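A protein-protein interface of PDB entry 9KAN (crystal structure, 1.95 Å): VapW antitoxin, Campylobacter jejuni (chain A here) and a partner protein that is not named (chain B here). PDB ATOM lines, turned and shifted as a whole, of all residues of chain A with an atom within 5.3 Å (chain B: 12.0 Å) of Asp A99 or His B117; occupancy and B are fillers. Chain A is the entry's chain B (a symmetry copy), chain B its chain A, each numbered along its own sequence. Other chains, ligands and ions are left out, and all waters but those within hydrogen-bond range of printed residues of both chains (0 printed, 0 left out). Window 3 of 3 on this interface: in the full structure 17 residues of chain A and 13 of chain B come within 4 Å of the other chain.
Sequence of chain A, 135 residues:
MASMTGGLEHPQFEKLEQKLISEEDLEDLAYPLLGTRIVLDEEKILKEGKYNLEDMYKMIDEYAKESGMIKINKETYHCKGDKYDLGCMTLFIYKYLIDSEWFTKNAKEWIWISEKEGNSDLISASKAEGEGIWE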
ATOM      1  N   ILE A  93      27.309 -12.683  13.018  1.00  0.00           N
ATOM      2  CA  ILE A  93      28.637 -12.269  13.459  1.00  0.00           C
ATOM      3  C   ILE A  93      28.575 -10.981  14.271  1.00  0.00           C
ATOM      4  O   ILE A  93      29.114 -10.896  15.379  1.00  0.00           O
ATOM      5  CB  ILE A  93      29.593 -12.134  12.243  1.00  0.00           C
ATOM      6  CG1 ILE A  93      29.871 -13.512  11.610  1.00  0.00           C
ATOM      7  CG2 ILE A  93      30.916 -11.562  12.675  1.00  0.00           C
ATOM      8  CD1 ILE A  93      28.955 -13.879  10.517  1.00  0.00           C
ATOM      9  N   TYR A  94      27.910  -9.961  13.751  1.00  0.00           N
ATOM     10  CA  TYR A  94      28.064  -8.634  14.307  1.00  0.00           C
ATOM     11  C   TYR A  94      26.891  -8.187  15.166  1.00  0.00           C
ATOM     12  O   TYR A  94      26.947  -7.095  15.728  1.00  0.00           O
ATOM     13  CB  TYR A  94      28.336  -7.632  13.186  1.00  0.00           C
ATOM     14  CG  TYR A  94      29.760  -7.750  12.713  1.00  0.00           C
ATOM     15  CD1 TYR A  94      30.821  -7.406  13.551  1.00  0.00           C
ATOM     16  CD2 TYR A  94      30.051  -8.233  11.452  1.00  0.00           C
ATOM     17  CE1 TYR A  94      32.128  -7.538  13.133  1.00  0.00           C
ATOM     18  CE2 TYR A  94      31.359  -8.355  11.019  1.00  0.00           C
ATOM     19  CZ  TYR A  94      32.394  -8.000  11.864  1.00  0.00           C
ATOM     20  OH  TYR A  94      33.702  -8.128  11.440  1.00  0.00           O
ATOM     21  N   LYS A  95      25.845  -8.999  15.305  1.00  0.00           N
ATOM     22  CA  LYS A  95      24.851  -8.772  16.347  1.00  0.00           C
ATOM     23  C   LYS A  95      24.977  -9.792  17.471  1.00  0.00           C
ATOM     24  O   LYS A  95      25.125  -9.410  18.633  1.00  0.00           O
ATOM     25  CB  LYS A  95      23.426  -8.792  15.784  1.00  0.00           C
ATOM     26  CG  LYS A  95      22.367  -8.641  16.884  1.00  0.00           C
ATOM     27  CD  LYS A  95      20.932  -8.662  16.360  1.00  0.00           C
ATOM     28  CE  LYS A  95      19.939  -8.372  17.499  1.00  0.00           C
ATOM     29  NZ  LYS A  95      18.505  -8.639  17.163  1.00  0.00           N
ATOM     30  N   TYR A  96      24.931 -11.089  17.152  1.00  0.00           N
ATOM     31  CA  TYR A  96      24.882 -12.094  18.215  1.00  0.00           C
ATOM     32  C   TYR A  96      26.266 -12.452  18.753  1.00  0.00           C
ATOM     33  O   TYR A  96      26.556 -12.225  19.932  1.00  0.00           O
ATOM     34  CB  TYR A  96      24.133 -13.341  17.736  1.00  0.00           C
ATOM     35  CG  TYR A  96      22.671 -13.072  17.472  1.00  0.00           C
ATOM     36  CD1 TYR A  96      21.840 -12.584  18.485  1.00  0.00           C
ATOM     37  CD2 TYR A  96      22.116 -13.315  16.221  1.00  0.00           C
ATOM     38  CE1 TYR A  96      20.498 -12.336  18.251  1.00  0.00           C
ATOM     39  CE2 TYR A  96      20.774 -13.069  15.981  1.00  0.00           C
ATOM     40  CZ  TYR A  96      19.968 -12.583  17.001  1.00  0.00           C
ATOM     41  OH  TYR A  96      18.630 -12.347  16.766  1.00  0.00           O
ATOM     42  N   LEU A  97      27.141 -13.012  17.910  1.00  0.00           N
ATOM     43  CA  LEU A  97      28.372 -13.605  18.435  1.00  0.00           C
ATOM     44  C   LEU A  97      29.319 -12.560  19.023  1.00  0.00           C
ATOM     45  O   LEU A  97      29.899 -12.785  20.093  1.00  0.00           O
ATOM     46  CB  LEU A  97      29.094 -14.402  17.351  1.00  0.00           C
ATOM     47  CG  LEU A  97      28.439 -15.742  17.001  1.00  0.00           C
ATOM     48  CD1 LEU A  97      28.967 -16.243  15.654  1.00  0.00           C
ATOM     49  CD2 LEU A  97      28.684 -16.764  18.108  1.00  0.00           C
ATOM     50  N   ILE A  98      29.497 -11.420  18.340  1.00  0.00           N
ATOM     51  CA  ILE A  98      30.561 -10.489  18.711  1.00  0.00           C
ATOM     52  C   ILE A  98      30.286  -9.844  20.066  1.00  0.00           C
ATOM     53  O   ILE A  98      31.220  -9.433  20.767  1.00  0.00           O
ATOM     54  CB  ILE A  98      30.748  -9.417  17.621  1.00  0.00           C
ATOM     55  CG1 ILE A  98      32.074  -8.677  17.823  1.00  0.00           C
ATOM     56  CG2 ILE A  98      29.572  -8.441  17.622  1.00  0.00           C
ATOM     57  CD1 ILE A  98      33.295  -9.565  17.769  1.00  0.00           C
ATOM     58  N   ASP A  99      29.016  -9.748  20.448  1.00  0.00           N
ATOM     59  CA  ASP A  99      28.582  -9.162  21.702  1.00  0.00           C
ATOM     60  C   ASP A  99      28.269 -10.213  22.754  1.00  0.00           C
ATOM     61  O   ASP A  99      27.708  -9.876  23.799  1.00  0.00           O
ATOM     62  CB  ASP A  99      27.371  -8.263  21.453  1.00  0.00           C
ATOM     63  CG  ASP A  99      27.742  -7.009  20.676  1.00  0.00           C
ATOM     64  OD1 ASP A  99      28.885  -6.514  20.865  1.00  0.00           O
ATOM     65  OD2 ASP A  99      26.909  -6.527  19.872  1.00  0.00           O
ATOM     66  N   SER A 100      28.616 -11.478  22.494  1.00  0.00           N
ATOM     67  CA  SER A 100      28.533 -12.559  23.471  1.00  0.00           C
ATOM     68  C   SER A 100      29.895 -12.704  24.141  1.00  0.00           C
ATOM     69  O   SER A 100      30.819 -13.275  23.555  1.00  0.00           O
ATOM     70  CB  SER A 100      28.118 -13.868  22.801  1.00  0.00           C
ATOM     71  OG  SER A 100      26.758 -13.838  22.406  1.00  0.00           O
ATOM     72  N   GLU A 101      30.015 -12.199  25.378  1.00  0.00           N
ATOM     73  CA  GLU A 101      31.309 -12.217  26.064  1.00  0.00           C
ATOM     74  C   GLU A 101      31.800 -13.645  26.313  1.00  0.00           C
ATOM     75  O   GLU A 101      32.981 -13.941  26.091  1.00  0.00           O
ATOM     76  CB  GLU A 101      31.228 -11.427  27.384  1.00  0.00           C
ATOM     77  CG  GLU A 101      32.604 -11.027  27.923  1.00  0.00           C
ATOM     78  CD  GLU A 101      32.573  -9.942  29.011  1.00  0.00           C
ATOM     79  OE1 GLU A 101      31.554  -9.235  29.166  1.00  0.00           O
ATOM     80  OE2 GLU A 101      33.590  -9.795  29.718  1.00  0.00           O
ATOM     81  N   THR A 104      33.415 -14.651  22.880  1.00  0.00           N
ATOM     82  CA  THR A 104      34.659 -14.062  22.395  1.00  0.00           C
ATOM     83  C   THR A 104      35.829 -14.379  23.320  1.00  0.00           C
ATOM     84  O   THR A 104      36.968 -14.532  22.858  1.00  0.00           O
ATOM     85  CB  THR A 104      34.499 -12.552  22.208  1.00  0.00           C
ATOM     86  OG1 THR A 104      33.927 -11.976  23.388  1.00  0.00           O
ATOM     87  CG2 THR A 104      33.596 -12.254  21.008  1.00  0.00           C
ATOM     88  N   GLY A 132      33.732  -6.322  20.400  1.00  0.00           N
ATOM     89  CA  GLY A 132      33.733  -7.426  21.347  1.00  0.00           C
ATOM     90  C   GLY A 132      34.709  -7.279  22.502  1.00  0.00           C
ATOM     91  O   GLY A 132      35.586  -6.409  22.474  1.00  0.00           O
ATOM     92  N   ASP B 110      16.005  -5.417  11.820  1.00  0.00           N
ATOM     93  CA  ASP B 110      16.409  -6.300  12.915  1.00  0.00           C
ATOM     94  C   ASP B 110      17.387  -5.613  13.852  1.00  0.00           C
ATOM     95  O   ASP B 110      17.254  -5.715  15.076  1.00  0.00           O
ATOM     96  CB  ASP B 110      17.048  -7.581  12.372  1.00  0.00           C
ATOM     97  CG  ASP B 110      16.028  -8.653  12.042  1.00  0.00           C
ATOM     98  OD1 ASP B 110      14.821  -8.338  12.033  1.00  0.00           O
ATOM     99  OD2 ASP B 110      16.437  -9.813  11.799  1.00  0.00           O
ATOM    100  N   LEU B 111      18.392  -4.935  13.295  1.00  0.00           N
ATOM    101  CA  LEU B 111      19.410  -4.306  14.127  1.00  0.00           C
ATOM    102  C   LEU B 111      18.793  -3.288  15.078  1.00  0.00           C
ATOM    103  O   LEU B 111      19.150  -3.237  16.260  1.00  0.00           O
ATOM    104  CB  LEU B 111      20.475  -3.654  13.245  1.00  0.00           C
ATOM    105  CG  LEU B 111      21.422  -4.601  12.503  1.00  0.00           C
ATOM    106  CD1 LEU B 111      22.158  -3.856  11.391  1.00  0.00           C
ATOM    107  CD2 LEU B 111      22.410  -5.290  13.455  1.00  0.00           C
ATOM    108  N   CYS B 112      17.823  -2.526  14.590  1.00  0.00           N
ATOM    109  CA  CYS B 112      17.180  -1.482  15.426  1.00  0.00           C
ATOM    110  C   CYS B 112      16.025  -2.104  16.235  1.00  0.00           C
ATOM    111  O   CYS B 112      14.981  -1.446  16.337  1.00  0.00           O
ATOM    112  CB  CYS B 112      16.681  -0.348  14.536  1.00  0.00           C
ATOM    113  SG  CYS B 112      17.856   0.234  13.289  1.00  0.00           S
ATOM    114  N   ALA B 113      16.225  -3.301  16.800  1.00  0.00           N
ATOM    115  CA  ALA B 113      15.173  -3.954  17.619  1.00  0.00           C
ATOM    116  C   ALA B 113      15.577  -3.968  19.097  1.00  0.00           C
ATOM    117  O   ALA B 113      14.691  -4.201  19.946  1.00  0.00           O
ATOM    118  CB  ALA B 113      14.898  -5.353  17.113  1.00  0.00           C
ATOM    119  N   LYS B 114      16.846  -3.731  19.400  1.00  0.00           N
ATOM    120  CA  LYS B 114      17.222  -3.649  20.832  1.00  0.00           C
ATOM    121  C   LYS B 114      16.425  -4.716  21.592  1.00  0.00           C
ATOM    122  O   LYS B 114      15.644  -4.349  22.499  1.00  0.00           O
ATOM    123  CB  LYS B 114      16.959  -2.240  21.370  1.00  0.00           C
ATOM    124  CG  LYS B 114      15.498  -1.825  21.318  1.00  0.00           C
ATOM    125  CD  LYS B 114      15.275  -0.419  21.861  1.00  0.00           C
ATOM    126  CE  LYS B 114      15.886   0.611  20.969  1.00  0.00           C
ATOM    127  NZ  LYS B 114      15.672   1.964  21.489  1.00  0.00           N
ATOM    128  N   ASP B 115      16.610  -5.982  21.223  1.00  0.00           N
ATOM    129  CA  ASP B 115      15.936  -7.079  21.971  1.00  0.00           C
ATOM    130  C   ASP B 115      17.041  -7.928  22.587  1.00  0.00           C
ATOM    131  O   ASP B 115      16.755  -8.692  23.525  1.00  0.00           O
ATOM    132  CB  ASP B 115      15.075  -7.938  21.067  1.00  0.00           C
ATOM    133  CG  ASP B 115      15.655  -8.223  19.688  1.00  0.00           C
ATOM    134  OD1 ASP B 115      16.808  -7.818  19.434  1.00  0.00           O
ATOM    135  OD2 ASP B 115      14.948  -8.853  18.878  1.00  0.00           O
ATOM    136  N   PHE B 116      18.244  -7.823  22.028  1.00  0.00           N
ATOM    137  CA  PHE B 116      19.422  -8.540  22.572  1.00  0.00           C
ATOM    138  C   PHE B 116      20.259  -7.455  23.207  1.00  0.00           C
ATOM    139  O   PHE B 116      20.557  -6.455  22.526  1.00  0.00           O
ATOM    140  CB  PHE B 116      20.020  -9.325  21.399  1.00  0.00           C
ATOM    141  CG  PHE B 116      21.304 -10.100  21.651  1.00  0.00           C
ATOM    142  CD1 PHE B 116      21.274 -11.354  22.246  1.00  0.00           C
ATOM    143  CD2 PHE B 116      22.534  -9.585  21.261  1.00  0.00           C
ATOM    144  CE1 PHE B 116      22.445 -12.061  22.461  1.00  0.00           C
ATOM    145  CE2 PHE B 116      23.699 -10.299  21.479  1.00  0.00           C
ATOM    146  CZ  PHE B 116      23.652 -11.534  22.076  1.00  0.00           C
ATOM    147  N   HIS B 117      20.618  -7.624  24.478  1.00  0.00           N
ATOM    148  CA  HIS B 117      21.307  -6.532  25.223  1.00  0.00           C
ATOM    149  C   HIS B 117      20.758  -5.155  24.838  1.00  0.00           C
ATOM    150  O   HIS B 117      20.012  -4.626  25.684  1.00  0.00           O
ATOM    151  CB  HIS B 117      22.820  -6.663  25.015  1.00  0.00           C
ATOM    152  CG  HIS B 117      23.336  -8.066  25.113  1.00  0.00           C
ATOM    153  ND1 HIS B 117      22.702  -9.076  25.805  1.00  0.00           N
ATOM    154  CD2 HIS B 117      24.446  -8.614  24.607  1.00  0.00           C
ATOM    155  CE1 HIS B 117      23.409 -10.191  25.702  1.00  0.00           C
ATOM    156  NE2 HIS B 117      24.474  -9.932  24.983  1.00  0.00           N
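The side-chain carboxylate (OD1) of Asp B115 is in salt-bridge range of the side-chain amino group (NZ) of Lys A95 (3.0 Å). A ring nitrogen (NE2) of His B117 is in hydrogen-bond range of the backbone carbonyl oxygen (O) of Asp A99 (3.4 Å).
Asp B110 touches Lys A95. CE2 of Phe B116 touches O of Lys A95, 3.3 Å away. Phe B116 touches Tyr A96 (CZ to O, 3.7 Å). Ser A100 touches Phe B116.
Asp A99 touches just one residue of chain B: His B117 (3.4 Å). His B117 touches just one residue of chain A: Asp A99. Printed residues of chain B within 4 Å of Lys A95: Asp B110 (3.8 Å), Asp B115 (3.0 Å) and Phe B116 (3.3 Å). Ser A100 touches one residue of chain B. No residue of chain B comes within 4 Å of Gly A132. Of the printed residues of chain A, Asp B110 touches Lys A95. Of the printed residues of chain A, Phe B116 touches Lys A95, Tyr A96 and Ser A100. Of the printed residues of chain A, Asp B115 touches Lys A95. Printed residues of chain B within 4 Å of Tyr A96: Phe B116. Leu B111 touches none of the printed residues of chain A. Ile A93 touches none of the printed residues of chain B. The nearest residue of chain B that does not touch Asp A99 is Phe B116 (4.2 Å).
The backbone carbonyl oxygen (O) of Ser A100 is in hydrogen-bond range of the side-chain hydroxyl (OG1) of Thr A104, at 3.4 Å. The backbone carbonyl oxygen of Tyr A96 lies within hydrogen-bond range of the side-chain hydroxyl of Ser A100, 3.0 Å away.
Hydrophobic or aromatic side chains of chain A that line the printed part of chain B: Tyr A96. Of the 8 printed residues of chain B, 4 touch a printed residue of chain A. Among the printed residues, 6 pairs touch across the chains.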
